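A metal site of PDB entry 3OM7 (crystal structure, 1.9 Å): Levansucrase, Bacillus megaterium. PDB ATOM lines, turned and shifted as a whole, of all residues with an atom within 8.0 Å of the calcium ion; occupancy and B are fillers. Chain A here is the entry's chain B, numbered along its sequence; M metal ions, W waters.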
ATOM      1  N   GLN A 208       3.931 -11.976  13.753  1.00  0.00           N
ATOM      2  CA  GLN A 208       3.877 -13.322  13.197  1.00  0.00           C
ATOM      3  C   GLN A 208       4.719 -13.430  11.923  1.00  0.00           C
ATOM      4  O   GLN A 208       4.762 -12.503  11.112  1.00  0.00           O
ATOM      5  CB  GLN A 208       2.412 -13.684  12.901  1.00  0.00           C
ATOM      6  CG  GLN A 208       2.155 -15.144  12.574  1.00  0.00           C
ATOM      7  CD  GLN A 208       0.740 -15.385  12.106  1.00  0.00           C
ATOM      8  OE1 GLN A 208       0.321 -14.878  11.066  1.00  0.00           O
ATOM      9  NE2 GLN A 208      -0.009 -16.160  12.876  1.00  0.00           N
ATOM     10  N   PHE A 213       2.699 -19.057  10.381  1.00  0.00           N
ATOM     11  CA  PHE A 213       1.457 -19.189   9.613  1.00  0.00           C
ATOM     12  C   PHE A 213       1.334 -20.580   8.976  1.00  0.00           C
ATOM     13  O   PHE A 213       0.298 -21.234   9.116  1.00  0.00           O
ATOM     14  CB  PHE A 213       1.372 -18.084   8.556  1.00  0.00           C
ATOM     15  CG  PHE A 213       0.322 -18.325   7.488  1.00  0.00           C
ATOM     16  CD1 PHE A 213      -1.007 -17.976   7.703  1.00  0.00           C
ATOM     17  CD2 PHE A 213       0.685 -18.866   6.259  1.00  0.00           C
ATOM     18  CE1 PHE A 213      -1.967 -18.183   6.720  1.00  0.00           C
ATOM     19  CE2 PHE A 213      -0.272 -19.085   5.270  1.00  0.00           C
ATOM     20  CZ  PHE A 213      -1.606 -18.744   5.496  1.00  0.00           C
ATOM     21  N   THR A 221      -7.370 -23.583   7.794  1.00  0.00           N
ATOM     22  CA  THR A 221      -8.255 -23.073   8.838  1.00  0.00           C
ATOM     23  C   THR A 221      -8.932 -21.741   8.476  1.00  0.00           C
ATOM     24  O   THR A 221      -9.933 -21.363   9.100  1.00  0.00           O
ATOM     25  CB  THR A 221      -7.515 -22.915  10.185  1.00  0.00           C
ATOM     26  OG1 THR A 221      -6.368 -22.072  10.014  1.00  0.00           O
ATOM     27  CG2 THR A 221      -7.068 -24.270  10.712  1.00  0.00           C
ATOM     28  N   GLY A 222      -8.400 -21.055   7.478  1.00  0.00           N
ATOM     29  CA  GLY A 222      -8.898 -19.732   7.097  1.00  0.00           C
ATOM     30  C   GLY A 222      -8.098 -18.621   7.751  1.00  0.00           C
ATOM     31  O   GLY A 222      -8.594 -17.501   7.906  1.00  0.00           O
ATOM     32  N   ASP A 223      -6.858 -18.930   8.142  1.00  0.00           N
ATOM     33  CA  ASP A 223      -5.954 -17.955   8.738  1.00  0.00           C
ATOM     34  C   ASP A 223      -5.385 -17.046   7.650  1.00  0.00           C
ATOM     35  O   ASP A 223      -5.360 -17.412   6.473  1.00  0.00           O
ATOM     36  CB  ASP A 223      -4.839 -18.657   9.513  1.00  0.00           C
ATOM     37  CG  ASP A 223      -4.139 -17.734  10.506  1.00  0.00           C
ATOM     38  OD1 ASP A 223      -4.705 -16.687  10.890  1.00  0.00           O
ATOM     39  OD2 ASP A 223      -3.013 -18.068  10.925  1.00  0.00           O
ATOM     40  N   ASN A 224      -4.931 -15.862   8.054  1.00  0.00           N
ATOM     41  CA  ASN A 224      -4.426 -14.858   7.127  1.00  0.00           C
ATOM     42  C   ASN A 224      -3.119 -14.219   7.622  1.00  0.00           C
ATOM     43  O   ASN A 224      -3.101 -13.576   8.673  1.00  0.00           O
ATOM     44  CB  ASN A 224      -5.490 -13.776   6.923  1.00  0.00           C
ATOM     45  CG  ASN A 224      -5.429 -13.149   5.554  1.00  0.00           C
ATOM     46  OD1 ASN A 224      -4.554 -12.319   5.278  1.00  0.00           O
ATOM     47  ND2 ASN A 224      -6.364 -13.526   4.691  1.00  0.00           N
ATOM     48  N   HIS A 225      -2.042 -14.410   6.857  1.00  0.00           N
ATOM     49  CA  HIS A 225      -0.737 -13.836   7.207  1.00  0.00           C
ATOM     50  C   HIS A 225      -0.474 -12.540   6.465  1.00  0.00           C
ATOM     51  O   HIS A 225      -0.564 -12.486   5.237  1.00  0.00           O
ATOM     52  CB  HIS A 225       0.400 -14.832   6.935  1.00  0.00           C
ATOM     53  CG  HIS A 225       1.759 -14.227   7.048  1.00  0.00           C
ATOM     54  ND1 HIS A 225       2.361 -13.976   8.261  1.00  0.00           N
ATOM     55  CD2 HIS A 225       2.645 -13.816   6.104  1.00  0.00           C
ATOM     56  CE1 HIS A 225       3.557 -13.433   8.061  1.00  0.00           C
ATOM     57  NE2 HIS A 225       3.746 -13.341   6.748  1.00  0.00           N
ATOM     58  N   THR A 226      -0.139 -11.490   7.218  1.00  0.00           N
ATOM     59  CA  THR A 226       0.139 -10.186   6.644  1.00  0.00           C
ATOM     60  C   THR A 226       1.405  -9.570   7.242  1.00  0.00           C
ATOM     61  O   THR A 226       1.659  -9.717   8.442  1.00  0.00           O
ATOM     62  CB  THR A 226      -1.024  -9.192   6.857  1.00  0.00           C
ATOM     63  OG1 THR A 226      -1.099  -8.833   8.242  1.00  0.00           O
ATOM     64  CG2 THR A 226      -2.353  -9.768   6.402  1.00  0.00           C
ATOM     65  N   ALA A 245       0.144  -6.068  10.094  1.00  0.00           N
ATOM     66  CA  ALA A 245       0.763  -7.298  10.559  1.00  0.00           C
ATOM     67  C   ALA A 245      -0.212  -8.159  11.362  1.00  0.00           C
ATOM     68  O   ALA A 245      -1.408  -7.877  11.432  1.00  0.00           O
ATOM     69  CB  ALA A 245       2.001  -6.976  11.388  1.00  0.00           C
ATOM     70  N   ASN A 246       0.322  -9.227  11.958  1.00  0.00           N
ATOM     71  CA  ASN A 246      -0.434 -10.042  12.898  1.00  0.00           C
ATOM     72  C   ASN A 246       0.408 -10.237  14.142  1.00  0.00           C
ATOM     73  O   ASN A 246       1.641 -10.215  14.063  1.00  0.00           O
ATOM     74  CB  ASN A 246      -0.809 -11.390  12.267  1.00  0.00           C
ATOM     75  CG  ASN A 246      -1.712 -11.233  11.059  1.00  0.00           C
ATOM     76  OD1 ASN A 246      -1.244 -11.131   9.925  1.00  0.00           O
ATOM     77  ND2 ASN A 246      -3.017 -11.201  11.295  1.00  0.00           N
ATOM     78  N   THR A 247      -0.246 -10.413  15.293  1.00  0.00           N
ATOM     79  CA  THR A 247       0.486 -10.565  16.549  1.00  0.00           C
ATOM     80  C   THR A 247       1.340 -11.825  16.540  1.00  0.00           C
ATOM     81  O   THR A 247       0.984 -12.818  15.889  1.00  0.00           O
ATOM     82  CB  THR A 247      -0.442 -10.614  17.786  1.00  0.00           C
ATOM     83  OG1 THR A 247      -1.371 -11.691  17.661  1.00  0.00           O
ATOM     84  CG2 THR A 247      -1.197  -9.280  17.966  1.00  0.00           C
ATOM     85  N   TYR A 253      -1.229 -13.675  21.014  1.00  0.00           N
ATOM     86  CA  TYR A 253      -1.303 -14.551  19.871  1.00  0.00           C
ATOM     87  C   TYR A 253      -2.721 -15.049  19.581  1.00  0.00           C
ATOM     88  O   TYR A 253      -3.591 -15.044  20.461  1.00  0.00           O
ATOM     89  CB  TYR A 253      -0.346 -15.738  20.072  1.00  0.00           C
ATOM     90  CG  TYR A 253       0.074 -16.422  18.785  1.00  0.00           C
ATOM     91  CD1 TYR A 253       0.563 -15.678  17.713  1.00  0.00           C
ATOM     92  CD2 TYR A 253      -0.003 -17.810  18.649  1.00  0.00           C
ATOM     93  CE1 TYR A 253       0.955 -16.290  16.543  1.00  0.00           C
ATOM     94  CE2 TYR A 253       0.397 -18.437  17.464  1.00  0.00           C
ATOM     95  CZ  TYR A 253       0.869 -17.663  16.422  1.00  0.00           C
ATOM     96  OH  TYR A 253       1.268 -18.239  15.234  1.00  0.00           O
ATOM     97  N   GLN A 254      -2.936 -15.465  18.327  1.00  0.00           N
ATOM     98  CA  GLN A 254      -4.169 -16.113  17.908  1.00  0.00           C
ATOM     99  C   GLN A 254      -4.393 -17.435  18.642  1.00  0.00           C
ATOM    100  O   GLN A 254      -3.447 -18.027  19.168  1.00  0.00           O
ATOM    101  CB  GLN A 254      -4.144 -16.354  16.393  1.00  0.00           C
ATOM    102  CG  GLN A 254      -2.973 -17.217  15.914  1.00  0.00           C
ATOM    103  CD  GLN A 254      -2.934 -17.385  14.409  1.00  0.00           C
ATOM    104  OE1 GLN A 254      -2.788 -18.508  13.907  1.00  0.00           O
ATOM    105  NE2 GLN A 254      -3.027 -16.284  13.675  1.00  0.00           N
ATOM    106  N   GLY A 255      -5.634 -17.874  18.660  1.00  0.00           N
ATOM    107  CA  GLY A 255      -6.022 -19.109  19.354  1.00  0.00           C
ATOM    108  C   GLY A 255      -7.302 -18.927  20.143  1.00  0.00           C
ATOM    109  O   GLY A 255      -7.842 -17.818  20.232  1.00  0.00           O
ATOM    110  N   LYS A 287     -13.203 -18.368  13.485  1.00  0.00           N
ATOM    111  CA  LYS A 287     -12.833 -17.128  12.804  1.00  0.00           C
ATOM    112  C   LYS A 287     -12.301 -16.066  13.762  1.00  0.00           C
ATOM    113  O   LYS A 287     -11.333 -15.377  13.447  1.00  0.00           O
ATOM    114  CB  LYS A 287     -14.033 -16.599  12.010  1.00  0.00           C
ATOM    115  CG  LYS A 287     -13.715 -15.490  11.024  1.00  0.00           C
ATOM    116  CD  LYS A 287     -14.927 -15.203  10.164  1.00  0.00           C
ATOM    117  CE  LYS A 287     -14.733 -13.972   9.300  1.00  0.00           C
ATOM    118  NZ  LYS A 287     -15.910 -13.754   8.420  1.00  0.00           N
ATOM    119  N   ALA A 288     -12.948 -15.931  14.921  1.00  0.00           N
ATOM    120  CA  ALA A 288     -12.520 -14.980  15.937  1.00  0.00           C
ATOM    121  C   ALA A 288     -11.197 -15.408  16.593  1.00  0.00           C
ATOM    122  O   ALA A 288     -10.298 -14.583  16.774  1.00  0.00           O
ATOM    123  CB  ALA A 288     -13.610 -14.802  16.991  1.00  0.00           C
ATOM    124  N   SER A 289     -11.080 -16.705  16.905  1.00  0.00           N
ATOM    125  CA  SER A 289      -9.850 -17.266  17.444  1.00  0.00           C
ATOM    126  C   SER A 289      -8.647 -16.972  16.550  1.00  0.00           C
ATOM    127  O   SER A 289      -7.578 -16.627  17.027  1.00  0.00           O
ATOM    128  CB  SER A 289      -9.995 -18.779  17.669  1.00  0.00           C
ATOM    129  OG  SER A 289     -11.100 -19.100  18.483  1.00  0.00           O
ATOM    130  N   LEU A 290      -8.842 -17.096  15.235  1.00  0.00           N
ATOM    131  CA  LEU A 290      -7.766 -16.902  14.267  1.00  0.00           C
ATOM    132  C   LEU A 290      -7.435 -15.427  14.035  1.00  0.00           C
ATOM    133  O   LEU A 290      -6.325 -15.102  13.583  1.00  0.00           O
ATOM    134  CB  LEU A 290      -8.090 -17.595  12.941  1.00  0.00           C
ATOM    135  CG  LEU A 290      -8.024 -19.119  12.931  1.00  0.00           C
ATOM    136  CD1 LEU A 290      -8.688 -19.652  11.683  1.00  0.00           C
ATOM    137  CD2 LEU A 290      -6.586 -19.636  13.042  1.00  0.00           C
ATOM    138  N   ALA A 291      -8.372 -14.557  14.367  1.00  0.00           N
ATOM    139  CA  ALA A 291      -8.224 -13.118  14.141  1.00  0.00           C
ATOM    140  C   ALA A 291      -7.253 -12.476  15.135  1.00  0.00           C
ATOM    141  O   ALA A 291      -7.534 -12.403  16.330  1.00  0.00           O
ATOM    142  CB  ALA A 291      -9.595 -12.438  14.216  1.00  0.00           C
ATOM    143  N   ASN A 292      -6.107 -12.043  14.625  1.00  0.00           N
ATOM    144  CA  ASN A 292      -5.115 -11.363  15.444  1.00  0.00           C
ATOM    145  C   ASN A 292      -4.415 -10.218  14.696  1.00  0.00           C
ATOM    146  O   ASN A 292      -3.198 -10.045  14.810  1.00  0.00           O
ATOM    147  CB  ASN A 292      -4.090 -12.357  16.044  1.00  0.00           C
ATOM    148  CG  ASN A 292      -3.149 -12.957  14.986  1.00  0.00           C
ATOM    149  OD1 ASN A 292      -3.513 -13.112  13.825  1.00  0.00           O
ATOM    150  ND2 ASN A 292      -1.941 -13.315  15.421  1.00  0.00           N
ATOM    151  N   GLY A 293      -5.183  -9.437  13.941  1.00  0.00           N
ATOM    152  CA  GLY A 293      -4.642  -8.315  13.174  1.00  0.00           C
ATOM    153  C   GLY A 293      -3.952  -7.285  14.050  1.00  0.00           C
ATOM    154  O   GLY A 293      -4.350  -7.060  15.198  1.00  0.00           O
ATOM    155  N   ASN A 317      -7.486  -8.275  17.817  1.00  0.00           N
ATOM    156  CA  ASN A 317      -7.762  -9.677  18.198  1.00  0.00           C
ATOM    157  C   ASN A 317      -9.255  -9.966  18.321  1.00  0.00           C
ATOM    158  O   ASN A 317     -10.013  -9.146  18.855  1.00  0.00           O
ATOM    159  CB  ASN A 317      -7.089 -10.046  19.520  1.00  0.00           C
ATOM    160  CG  ASN A 317      -5.577 -10.212  19.396  1.00  0.00           C
ATOM    161  OD1 ASN A 317      -4.847  -9.233  19.258  1.00  0.00           O
ATOM    162  ND2 ASN A 317      -5.119 -11.443  19.497  1.00  0.00           N
ATOM    163  N   THR A 320     -10.885  -9.033  13.725  1.00  0.00           N
ATOM    164  CA  THR A 320     -10.469  -9.335  12.352  1.00  0.00           C
ATOM    165  C   THR A 320      -9.001  -9.702  12.239  1.00  0.00           C
ATOM    166  O   THR A 320      -8.179  -9.305  13.060  1.00  0.00           O
ATOM    167  CB  THR A 320     -10.799  -8.181  11.373  1.00  0.00           C
ATOM    168  OG1 THR A 320     -10.402  -8.543  10.041  1.00  0.00           O
ATOM    169  CG2 THR A 320     -10.078  -6.897  11.773  1.00  0.00           C
ATOM    170  N   ASP A 321      -8.681 -10.488  11.220  1.00  0.00           N
ATOM    171  CA  ASP A 321      -7.306 -10.846  10.939  1.00  0.00           C
ATOM    172  C   ASP A 321      -6.655  -9.822  10.013  1.00  0.00           C
ATOM    173  O   ASP A 321      -5.448  -9.822   9.833  1.00  0.00           O
ATOM    174  CB  ASP A 321      -7.239 -12.231  10.306  1.00  0.00           C
ATOM    175  CG  ASP A 321      -6.048 -13.030  10.788  1.00  0.00           C
ATOM    176  OD1 ASP A 321      -5.785 -14.109  10.207  1.00  0.00           O
ATOM    177  OD2 ASP A 321      -5.367 -12.599  11.747  1.00  0.00           O
ATOM    178  N   GLU A 322      -7.474  -8.943   9.437  1.00  0.00           N
ATOM    179  CA  GLU A 322      -7.004  -8.021   8.409  1.00  0.00           C
ATOM    180  C   GLU A 322      -7.399  -6.564   8.626  1.00  0.00           C
ATOM    181  O   GLU A 322      -8.507  -6.143   8.274  1.00  0.00           O
ATOM    182  CB  GLU A 322      -7.434  -8.486   7.009  1.00  0.00           C
ATOM    183  CG  GLU A 322      -6.638  -9.676   6.496  1.00  0.00           C
ATOM    184  CD  GLU A 322      -6.667  -9.798   4.988  1.00  0.00           C
ATOM    185  OE1 GLU A 322      -7.051 -10.867   4.484  1.00  0.00           O
ATOM    186  OE2 GLU A 322      -6.287  -8.827   4.307  1.00  0.00           O
HETATM  187 CA    CA M   1      -4.339 -14.825  12.372  1.00  0.00          CA
HETATM  188  O   HOH W   1      -2.445 -14.348  11.020  1.00  0.00           O
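The calcium ion is bound by the backbone carbonyl oxygen (O) of Leu 290 (2.3 Å). NE2 of Gln 254 binds the calcium ion (2.4 Å). The calcium ion is bound by water W1 (2.4 Å). The calcium ion is bound by OD1 of Asn 292 (2.4 Å). The side-chain carboxylate (OD1) of Asp 223 binds the calcium ion, at 2.4 Å. The side-chain carboxylate (OD2) of Asp 321 is bound to the calcium ion (2.5 Å). The calcium ion is bound by OD1 of Asp 321. The calcium ion has seven donor atoms within binding distance.
Water W1 lies within hydrogen-bond range of the backbone carbonyl oxygen (O) of Asn 224, the side-chain amide oxygen (OE1) of Gln 208 and the side-chain amide nitrogen (ND2) of Asn 246.
The side-chain amide nitrogen (NE2) of Gln 208 lies close to the side-chain amide nitrogen (NE2) of Gln 254 (3.1 Å). ND2 of Asn 246 lies close to OD1 of Asn 292 (3.2 Å). The side-chain amide nitrogen (ND2) of Asn 292 sits at hydrogen-bond distance from the side-chain hydroxyl (OG1) of Thr 247. The backbone carbonyl oxygen (O) of Asp 321 lies within hydrogen-bond range of the side-chain amide nitrogen (ND2) of Asn 246, at 3.2 Å. The backbone NH of Asn 224 sits close to the side-chain carboxylate of Asp 321, 2.9 Å away.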
